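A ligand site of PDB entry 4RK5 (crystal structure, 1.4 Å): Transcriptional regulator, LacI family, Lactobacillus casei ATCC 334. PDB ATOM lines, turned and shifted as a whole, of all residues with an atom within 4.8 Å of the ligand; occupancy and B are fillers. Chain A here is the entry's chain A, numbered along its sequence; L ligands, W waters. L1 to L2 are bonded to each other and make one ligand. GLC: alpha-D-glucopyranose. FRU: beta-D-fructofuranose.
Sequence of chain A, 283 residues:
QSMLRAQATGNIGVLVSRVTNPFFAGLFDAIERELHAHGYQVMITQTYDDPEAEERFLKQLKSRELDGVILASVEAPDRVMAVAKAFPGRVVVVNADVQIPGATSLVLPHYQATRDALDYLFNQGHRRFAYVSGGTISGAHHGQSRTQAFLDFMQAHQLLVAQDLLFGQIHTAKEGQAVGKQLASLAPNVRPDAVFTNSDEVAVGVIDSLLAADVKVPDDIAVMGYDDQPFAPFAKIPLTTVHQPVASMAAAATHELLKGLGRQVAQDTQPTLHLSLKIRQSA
ND2 of Asn 21 lies within hydrogen-bond range of O6 of GLC L1, at 3.0 Å.
O3 of GLC L1 sits at hydrogen-bond distance from ND2 of Asn 95 (3.5 Å).
NE2 of Gln 244 sits at hydrogen-bond distance from O3 of GLC L1 (3.0 Å).
The side-chain carboxylate (OD2) of Asp 227 is in hydrogen-bond range of an oxygen (O6) of GLC L1 (2.6 Å).
O6 of FRU L2 sits at hydrogen-bond distance from NH2 of Arg 18, 3.3 Å away.
The guanidinium group (NH2) of Arg 146 lies within hydrogen-bond range of an oxygen (O4) of GLC L1, at 2.9 Å.
The side-chain hydroxyl (OG) of Ser 17 lies within hydrogen-bond range of an oxygen (O1) of FRU L2 (3.1 Å).
NE2 of His 142 lies within hydrogen-bond range of OE2 of Glu 75 (2.9 Å).
OD1 of Asn 21 is in hydrogen-bond range of NE2 of Gln 229, at 3.5 Å.
ND1 of His 110 is in hydrogen-bond range of NH2 of Arg 146.
The side-chain carboxylate (OD2) of Asp 227 sits at hydrogen-bond distance from the side-chain amide nitrogen (NE2) of Gln 229.
OD1 of Asn 21 sits at hydrogen-bond distance from N of Phe 23 (2.9 Å).
NH1 of Arg 146 is in hydrogen-bond range of OD1 of Asn 198 (3.0 Å).
NE2 of Gln 244 lies within hydrogen-bond range of OD1 of Asp 227.
The side-chain amide oxygen (OD1) of Asn 95 sits at hydrogen-bond distance from a ring nitrogen (NE2) of His 110, at 2.8 Å.
Merely in contact with the ligand: Phe 24 (3.6 Å), Asp 49 (3.8 Å), Ser 73 (3.9 Å), Gly 134 (3.3 Å), His 142 (3.4 Å), His 171 (3.2 Å), Asn 198 (3.7 Å), Tyr 226 (3.8 Å) and Gln 229 (3.7 Å).
Hydrophobic or aromatic side chains that line the ligand: Phe 24, His 142, His 171 and Tyr 226.
16 residues have an atom within 4 Å of the ligand: Ser 17, Arg 18, Asn 21, Phe 24, Asp 49, Ser 73, Asn 95, Gly 134, His 142, Arg 146, His 171, Asn 198, Tyr 226, Asp 227, Gln 229 and Gln 244.
The nearest printed residue that does not touch the ligand is Phe 23 (4.01 Å).
Water W6 bridges O3 of FRU L2 (2.7 Å) and NH1 of Arg 146 (3.5 Å).
Water W2 lies within hydrogen-bond range of the side-chain hydroxyl of Ser 199 (2.6 Å), an oxygen (O6) of GLC L1 (2.7 Å), the side-chain amide nitrogen of Gln 229 (3.2 Å) and the side-chain amide oxygen of Asn 21 (3.5 Å).
Water W8 lies within hydrogen-bond range of an oxygen (O3) of GLC L1 (2.8 Å) and the backbone carbonyl oxygen (O) of Asn 95 (2.9 Å).
Water W9 bridges the backbone carbonyl oxygen of Ala 72 (2.9 Å) and an oxygen (O2) of GLC L1 (3.2 Å).
Water W1 lies within hydrogen-bond range of the backbone carbonyl oxygen of His 171 (2.7 Å), the side-chain hydroxyl of Ser 199 (3.4 Å) and the guanidinium group of Arg 18 (3.5 Å).
Water W7 bridges the side-chain carboxylate (OD2) of Asp 49 (2.6 Å) and an oxygen (O4) of FRU L2 (3.3 Å).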
ATOM      1  N   SER A  17      29.440 -16.831  -9.708  1.00  0.00           N
ATOM      2  CA  SER A  17      30.554 -15.981 -10.087  1.00  0.00           C
ATOM      3  C   SER A  17      31.839 -16.147  -9.249  1.00  0.00           C
ATOM      4  O   SER A  17      32.910 -16.041  -9.771  1.00  0.00           O
ATOM      5  CB  SER A  17      30.132 -14.533 -10.294  1.00  0.00           C
ATOM      6  OG  SER A  17      29.770 -13.958  -9.082  1.00  0.00           O
ATOM      7  N   ARG A  18      31.711 -16.370  -7.938  1.00  0.00           N
ATOM      8  CA  ARG A  18      32.895 -16.379  -7.044  1.00  0.00           C
ATOM      9  C   ARG A  18      32.585 -17.160  -5.776  1.00  0.00           C
ATOM     10  O   ARG A  18      31.681 -16.777  -5.042  1.00  0.00           O
ATOM     11  CB  ARG A  18      33.331 -14.952  -6.744  1.00  0.00           C
ATOM     12  CG  ARG A  18      34.518 -14.852  -5.820  1.00  0.00           C
ATOM     13  CD  ARG A  18      35.070 -13.418  -5.713  1.00  0.00           C
ATOM     14  NE  ARG A  18      34.088 -12.480  -5.306  1.00  0.00           N
ATOM     15  CZ  ARG A  18      33.805 -12.165  -4.036  1.00  0.00           C
ATOM     16  NH1 ARG A  18      34.475 -12.661  -3.004  1.00  0.00           N
ATOM     17  NH2 ARG A  18      32.847 -11.274  -3.808  1.00  0.00           N
ATOM     18  N   ASN A  21      32.777 -15.502  -2.235  1.00  0.00           N
ATOM     19  CA  ASN A  21      31.641 -14.709  -1.775  1.00  0.00           C
ATOM     20  C   ASN A  21      30.855 -15.608  -0.817  1.00  0.00           C
ATOM     21  O   ASN A  21      30.291 -16.629  -1.253  1.00  0.00           O
ATOM     22  CB  ASN A  21      30.790 -14.310  -2.968  1.00  0.00           C
ATOM     23  CG  ASN A  21      29.575 -13.538  -2.584  1.00  0.00           C
ATOM     24  OD1 ASN A  21      29.108 -13.602  -1.446  1.00  0.00           O
ATOM     25  ND2 ASN A  21      28.990 -12.880  -3.560  1.00  0.00           N
ATOM     26  N   PHE A  23      27.992 -15.534   0.419  1.00  0.00           N
ATOM     27  CA  PHE A  23      26.642 -15.789  -0.033  1.00  0.00           C
ATOM     28  C   PHE A  23      26.619 -17.028  -0.952  1.00  0.00           C
ATOM     29  O   PHE A  23      25.786 -17.939  -0.790  1.00  0.00           O
ATOM     30  CB  PHE A  23      26.053 -14.580  -0.751  1.00  0.00           C
ATOM     31  CG  PHE A  23      24.762 -14.899  -1.453  1.00  0.00           C
ATOM     32  CD1 PHE A  23      23.574 -14.996  -0.721  1.00  0.00           C
ATOM     33  CD2 PHE A  23      24.733 -15.142  -2.790  1.00  0.00           C
ATOM     34  CE1 PHE A  23      22.449 -15.396  -1.340  1.00  0.00           C
ATOM     35  CE2 PHE A  23      23.561 -15.543  -3.402  1.00  0.00           C
ATOM     36  CZ  PHE A  23      22.415 -15.664  -2.657  1.00  0.00           C
ATOM     37  N   PHE A  24      27.525 -17.055  -1.927  1.00  0.00           N
ATOM     38  CA  PHE A  24      27.540 -18.189  -2.842  1.00  0.00           C
ATOM     39  C   PHE A  24      28.027 -19.463  -2.145  1.00  0.00           C
ATOM     40  O   PHE A  24      27.489 -20.537  -2.444  1.00  0.00           O
ATOM     41  CB  PHE A  24      28.403 -17.879  -4.065  1.00  0.00           C
ATOM     42  CG  PHE A  24      27.775 -17.002  -5.109  1.00  0.00           C
ATOM     43  CD1 PHE A  24      26.486 -17.235  -5.569  1.00  0.00           C
ATOM     44  CD2 PHE A  24      28.469 -15.935  -5.656  1.00  0.00           C
ATOM     45  CE1 PHE A  24      25.942 -16.478  -6.575  1.00  0.00           C
ATOM     46  CE2 PHE A  24      27.886 -15.159  -6.662  1.00  0.00           C
ATOM     47  CZ  PHE A  24      26.631 -15.467  -7.117  1.00  0.00           C
ATOM     48  N   ASP A  49      32.530 -13.872 -13.856  1.00  0.00           N
ATOM     49  CA  ASP A  49      31.743 -13.107 -14.887  1.00  0.00           C
ATOM     50  C   ASP A  49      32.207 -13.307 -16.331  1.00  0.00           C
ATOM     51  O   ASP A  49      31.832 -12.539 -17.210  1.00  0.00           O
ATOM     52  CB  ASP A  49      31.782 -11.615 -14.603  1.00  0.00           C
ATOM     53  CG  ASP A  49      31.114 -11.282 -13.304  1.00  0.00           C
ATOM     54  OD1 ASP A  49      30.160 -12.006 -12.940  1.00  0.00           O
ATOM     55  OD2 ASP A  49      31.589 -10.350 -12.617  1.00  0.00           O
ATOM     56  N   ALA A  72      23.406 -19.878 -10.247  1.00  0.00           N
ATOM     57  CA  ALA A  72      23.044 -18.798  -9.361  1.00  0.00           C
ATOM     58  C   ALA A  72      23.563 -17.446  -9.855  1.00  0.00           C
ATOM     59  O   ALA A  72      23.391 -16.397  -9.186  1.00  0.00           O
ATOM     60  CB  ALA A  72      23.510 -19.052  -7.924  1.00  0.00           C
ATOM     61  N   SER A  73      24.197 -17.451 -11.034  1.00  0.00           N
ATOM     62  CA  SER A  73      24.558 -16.285 -11.776  1.00  0.00           C
ATOM     63  C   SER A  73      24.503 -16.657 -13.237  1.00  0.00           C
ATOM     64  O   SER A  73      24.706 -17.792 -13.579  1.00  0.00           O
ATOM     65  CB  SER A  73      25.893 -15.763 -11.318  1.00  0.00           C
ATOM     66  OG  SER A  73      26.872 -16.702 -11.358  1.00  0.00           O
ATOM     67  N   GLU A  75      25.593 -15.104 -17.218  1.00  0.00           N
ATOM     68  CA  GLU A  75      26.332 -14.137 -18.030  1.00  0.00           C
ATOM     69  C   GLU A  75      25.696 -13.880 -19.379  1.00  0.00           C
ATOM     70  O   GLU A  75      25.569 -12.723 -19.807  1.00  0.00           O
ATOM     71  CB  GLU A  75      27.765 -14.626 -18.217  1.00  0.00           C
ATOM     72  CG  GLU A  75      28.467 -14.787 -16.912  1.00  0.00           C
ATOM     73  CD  GLU A  75      28.332 -13.565 -15.948  1.00  0.00           C
ATOM     74  OE1 GLU A  75      28.373 -12.409 -16.447  1.00  0.00           O
ATOM     75  OE2 GLU A  75      28.166 -13.817 -14.685  1.00  0.00           O
ATOM     76  N   ASN A  95      17.943 -16.895  -8.393  1.00  0.00           N
ATOM     77  CA  ASN A  95      18.380 -15.615  -7.839  1.00  0.00           C
ATOM     78  C   ASN A  95      19.365 -14.850  -8.723  1.00  0.00           C
ATOM     79  O   ASN A  95      20.219 -14.143  -8.215  1.00  0.00           O
ATOM     80  CB  ASN A  95      18.952 -15.825  -6.431  1.00  0.00           C
ATOM     81  CG  ASN A  95      18.987 -14.549  -5.630  1.00  0.00           C
ATOM     82  OD1 ASN A  95      18.086 -13.710  -5.741  1.00  0.00           O
ATOM     83  ND2 ASN A  95      20.011 -14.407  -4.809  1.00  0.00           N
ATOM     84  N   HIS A 110      14.607  -8.085  -5.517  1.00  0.00           N
ATOM     85  CA  HIS A 110      15.675  -7.202  -5.128  1.00  0.00           C
ATOM     86  C   HIS A 110      15.400  -5.719  -5.336  1.00  0.00           C
ATOM     87  O   HIS A 110      15.878  -4.903  -4.579  1.00  0.00           O
ATOM     88  CB  HIS A 110      16.978  -7.615  -5.773  1.00  0.00           C
ATOM     89  CG  HIS A 110      17.460  -8.935  -5.282  1.00  0.00           C
ATOM     90  ND1 HIS A 110      18.072  -9.094  -4.056  1.00  0.00           N
ATOM     91  CD2 HIS A 110      17.429 -10.163  -5.859  1.00  0.00           C
ATOM     92  CE1 HIS A 110      18.387 -10.373  -3.906  1.00  0.00           C
ATOM     93  NE2 HIS A 110      18.005 -11.043  -4.983  1.00  0.00           N
ATOM     94  N   GLY A 134      28.732  -4.019  -7.657  1.00  0.00           N
ATOM     95  CA  GLY A 134      29.673  -4.918  -8.230  1.00  0.00           C
ATOM     96  C   GLY A 134      29.787  -4.811  -9.740  1.00  0.00           C
ATOM     97  O   GLY A 134      30.709  -5.387 -10.301  1.00  0.00           O
ATOM     98  N   GLY A 135      28.893  -4.099 -10.362  1.00  0.00           N
ATOM     99  CA  GLY A 135      28.922  -3.870 -11.788  1.00  0.00           C
ATOM    100  C   GLY A 135      29.388  -2.485 -12.145  1.00  0.00           C
ATOM    101  O   GLY A 135      29.770  -1.672 -11.292  1.00  0.00           O
ATOM    102  N   HIS A 142      25.256  -6.923 -13.799  1.00  0.00           N
ATOM    103  CA  HIS A 142      24.643  -7.624 -12.686  1.00  0.00           C
ATOM    104  C   HIS A 142      24.306  -6.729 -11.528  1.00  0.00           C
ATOM    105  O   HIS A 142      25.053  -5.794 -11.136  1.00  0.00           O
ATOM    106  CB  HIS A 142      25.489  -8.757 -12.184  1.00  0.00           C
ATOM    107  CG  HIS A 142      25.799  -9.740 -13.236  1.00  0.00           C
ATOM    108  ND1 HIS A 142      25.705  -9.456 -14.581  1.00  0.00           N
ATOM    109  CD2 HIS A 142      26.249 -11.016 -13.149  1.00  0.00           C
ATOM    110  CE1 HIS A 142      26.049 -10.537 -15.265  1.00  0.00           C
ATOM    111  NE2 HIS A 142      26.405 -11.478 -14.428  1.00  0.00           N
ATOM    112  N   GLY A 143      23.151  -7.025 -10.989  1.00  0.00           N
ATOM    113  CA  GLY A 143      22.593  -6.205  -9.868  1.00  0.00           C
ATOM    114  C   GLY A 143      21.955  -4.914 -10.378  1.00  0.00           C
ATOM    115  O   GLY A 143      21.813  -3.950  -9.668  1.00  0.00           O
ATOM    116  N   ARG A 146      18.809  -3.469  -8.645  1.00  0.00           N
ATOM    117  CA  ARG A 146      19.196  -2.685  -7.479  1.00  0.00           C
ATOM    118  C   ARG A 146      19.619  -1.240  -7.847  1.00  0.00           C
ATOM    119  O   ARG A 146      19.254  -0.281  -7.188  1.00  0.00           O
ATOM    120  CB  ARG A 146      20.269  -3.368  -6.667  1.00  0.00           C
ATOM    121  CG  ARG A 146      19.888  -4.756  -6.255  1.00  0.00           C
ATOM    122  CD  ARG A 146      20.993  -5.376  -5.568  1.00  0.00           C
ATOM    123  NE  ARG A 146      20.813  -6.780  -5.431  1.00  0.00           N
ATOM    124  CZ  ARG A 146      21.669  -7.569  -4.753  1.00  0.00           C
ATOM    125  NH1 ARG A 146      22.703  -7.028  -4.087  1.00  0.00           N
ATOM    126  NH2 ARG A 146      21.491  -8.852  -4.692  1.00  0.00           N
ATOM    127  N   HIS A 171      33.707  -5.506  -5.105  1.00  0.00           N
ATOM    128  CA  HIS A 171      33.222  -6.837  -4.725  1.00  0.00           C
ATOM    129  C   HIS A 171      33.669  -7.310  -3.361  1.00  0.00           C
ATOM    130  O   HIS A 171      32.895  -7.960  -2.625  1.00  0.00           O
ATOM    131  CB  HIS A 171      33.705  -7.877  -5.749  1.00  0.00           C
ATOM    132  CG  HIS A 171      33.314  -7.604  -7.134  1.00  0.00           C
ATOM    133  ND1 HIS A 171      34.190  -7.199  -8.097  1.00  0.00           N
ATOM    134  CD2 HIS A 171      32.104  -7.591  -7.710  1.00  0.00           C
ATOM    135  CE1 HIS A 171      33.511  -6.959  -9.215  1.00  0.00           C
ATOM    136  NE2 HIS A 171      32.251  -7.196  -8.995  1.00  0.00           N
ATOM    137  N   ASN A 198      25.781  -2.911  -1.356  1.00  0.00           N
ATOM    138  CA  ASN A 198      25.430  -4.060  -2.189  1.00  0.00           C
ATOM    139  C   ASN A 198      26.098  -5.370  -1.774  1.00  0.00           C
ATOM    140  O   ASN A 198      25.957  -6.379  -2.495  1.00  0.00           O
ATOM    141  CB  ASN A 198      25.633  -3.761  -3.675  1.00  0.00           C
ATOM    142  CG  ASN A 198      24.365  -3.426  -4.377  1.00  0.00           C
ATOM    143  OD1 ASN A 198      23.363  -4.139  -4.247  1.00  0.00           O
ATOM    144  ND2 ASN A 198      24.357  -2.339  -5.125  1.00  0.00           N
ATOM    145  N   SER A 199      26.757  -5.404  -0.614  1.00  0.00           N
ATOM    146  CA  SER A 199      27.458  -6.628  -0.251  1.00  0.00           C
ATOM    147  C   SER A 199      28.009  -6.478   1.171  1.00  0.00           C
ATOM    148  O   SER A 199      28.700  -5.520   1.521  1.00  0.00           O
ATOM    149  CB  SER A 199      28.692  -6.815  -1.147  1.00  0.00           C
ATOM    150  OG  SER A 199      29.661  -7.635  -0.536  1.00  0.00           O
ATOM    151  N   TYR A 226      24.529  -5.991   2.298  1.00  0.00           N
ATOM    152  CA  TYR A 226      23.541  -6.771   1.562  1.00  0.00           C
ATOM    153  C   TYR A 226      23.910  -8.230   1.678  1.00  0.00           C
ATOM    154  O   TYR A 226      25.077  -8.596   1.463  1.00  0.00           O
ATOM    155  CB  TYR A 226      23.484  -6.383   0.071  1.00  0.00           C
ATOM    156  CG  TYR A 226      22.116  -6.527  -0.587  1.00  0.00           C
ATOM    157  CD1 TYR A 226      21.590  -7.776  -0.902  1.00  0.00           C
ATOM    158  CD2 TYR A 226      21.349  -5.449  -0.907  1.00  0.00           C
ATOM    159  CE1 TYR A 226      20.355  -7.891  -1.497  1.00  0.00           C
ATOM    160  CE2 TYR A 226      20.152  -5.524  -1.560  1.00  0.00           C
ATOM    161  CZ  TYR A 226      19.630  -6.769  -1.835  1.00  0.00           C
ATOM    162  OH  TYR A 226      18.417  -6.862  -2.471  1.00  0.00           O
ATOM    163  N   ASP A 227      22.928  -9.044   2.042  1.00  0.00           N
ATOM    164  CA  ASP A 227      22.888 -10.527   2.003  1.00  0.00           C
ATOM    165  C   ASP A 227      22.576 -11.133   3.381  1.00  0.00           C
ATOM    166  O   ASP A 227      21.866 -12.145   3.431  1.00  0.00           O
ATOM    167  CB  ASP A 227      24.144 -11.222   1.499  1.00  0.00           C
ATOM    168  CG  ASP A 227      24.456 -10.974   0.023  1.00  0.00           C
ATOM    169  OD1 ASP A 227      23.589 -10.474  -0.709  1.00  0.00           O
ATOM    170  OD2 ASP A 227      25.594 -11.335  -0.311  1.00  0.00           O
ATOM    171  N   GLN A 229      25.194 -12.281   5.397  1.00  0.00           N
ATOM    172  CA  GLN A 229      26.166 -13.340   5.362  1.00  0.00           C
ATOM    173  C   GLN A 229      26.516 -13.827   6.776  1.00  0.00           C
ATOM    174  O   GLN A 229      26.255 -13.141   7.753  1.00  0.00           O
ATOM    175  CB  GLN A 229      27.440 -12.889   4.614  1.00  0.00           C
ATOM    176  CG  GLN A 229      27.138 -12.617   3.157  1.00  0.00           C
ATOM    177  CD  GLN A 229      28.302 -12.029   2.384  1.00  0.00           C
ATOM    178  OE1 GLN A 229      29.444 -12.002   2.857  1.00  0.00           O
ATOM    179  NE2 GLN A 229      28.015 -11.565   1.171  1.00  0.00           N
ATOM    180  N   GLN A 244      18.987 -12.253   2.679  1.00  0.00           N
ATOM    181  CA  GLN A 244      18.558 -13.193   1.636  1.00  0.00           C
ATOM    182  C   GLN A 244      18.257 -14.546   2.275  1.00  0.00           C
ATOM    183  O   GLN A 244      19.047 -15.040   3.080  1.00  0.00           O
ATOM    184  CB  GLN A 244      19.618 -13.353   0.544  1.00  0.00           C
ATOM    185  CG  GLN A 244      19.878 -12.066  -0.232  1.00  0.00           C
ATOM    186  CD  GLN A 244      20.318 -12.317  -1.650  1.00  0.00           C
ATOM    187  OE1 GLN A 244      19.580 -12.979  -2.396  1.00  0.00           O
ATOM    188  NE2 GLN A 244      21.454 -11.797  -2.027  1.00  0.00           N
HETATM  189  C1  GLC L   1      26.023 -11.998  -6.108  1.00  0.00           C
HETATM  190  C2  GLC L   1      24.616 -12.483  -5.784  1.00  0.00           C
HETATM  191  C3  GLC L   1      23.763 -11.395  -5.158  1.00  0.00           C
HETATM  192  C4  GLC L   1      24.497 -10.928  -3.908  1.00  0.00           C
HETATM  193  C5  GLC L   1      25.856 -10.378  -4.342  1.00  0.00           C
HETATM  194  C6  GLC L   1      26.748  -9.868  -3.227  1.00  0.00           C
HETATM  195  O2  GLC L   1      24.005 -12.980  -7.007  1.00  0.00           O
HETATM  196  O3  GLC L   1      22.491 -11.938  -4.791  1.00  0.00           O
HETATM  197  O4  GLC L   1      23.763  -9.878  -3.266  1.00  0.00           O
HETATM  198  O5  GLC L   1      26.638 -11.432  -4.980  1.00  0.00           O
HETATM  199  O6  GLC L   1      27.128 -10.934  -2.328  1.00  0.00           O
HETATM  200  C1  FRU L   2      26.419 -12.110  -9.294  1.00  0.00           C
HETATM  201  C2  FRU L   2      26.908 -11.150  -8.212  1.00  0.00           C
HETATM  202  C3  FRU L   2      27.231  -9.732  -8.663  1.00  0.00           C
HETATM  203  C4  FRU L   2      28.212  -9.291  -7.590  1.00  0.00           C
HETATM  204  C5  FRU L   2      29.068 -10.539  -7.466  1.00  0.00           C
HETATM  205  C6  FRU L   2      29.733 -10.721  -6.133  1.00  0.00           C
HETATM  206  O1  FRU L   2      27.435 -12.335 -10.290  1.00  0.00           O
HETATM  207  O2  FRU L   2      25.921 -11.024  -7.174  1.00  0.00           O
HETATM  208  O3  FRU L   2      26.048  -8.924  -8.787  1.00  0.00           O
HETATM  209  O4  FRU L   2      28.976  -8.159  -7.974  1.00  0.00           O
HETATM  210  O5  FRU L   2      28.142 -11.642  -7.701  1.00  0.00           O
HETATM  211  O6  FRU L   2      30.496 -11.902  -6.007  1.00  0.00           O
HETATM  212  O   HOH W   1      30.524  -8.730  -3.604  1.00  0.00           O
HETATM  213  O   HOH W   2      29.476 -10.175  -1.263  1.00  0.00           O
HETATM  214  O   HOH W   3      28.899  -6.991  -5.074  1.00  0.00           O
HETATM  215  O   HOH W   4      22.908 -10.938  -8.742  1.00  0.00           O
HETATM  216  O   HOH W   5      22.433 -15.236  -6.875  1.00  0.00           O
HETATM  217  O   HOH W   6      24.212  -8.168  -6.982  1.00  0.00           O
HETATM  218  O   HOH W   7      29.864  -9.362 -10.965  1.00  0.00           O
HETATM  219  O   HOH W   8      20.816 -11.639  -6.988  1.00  0.00           O
HETATM  220  O   HOH W   9      23.285 -13.632 -10.021  1.00  0.00           O
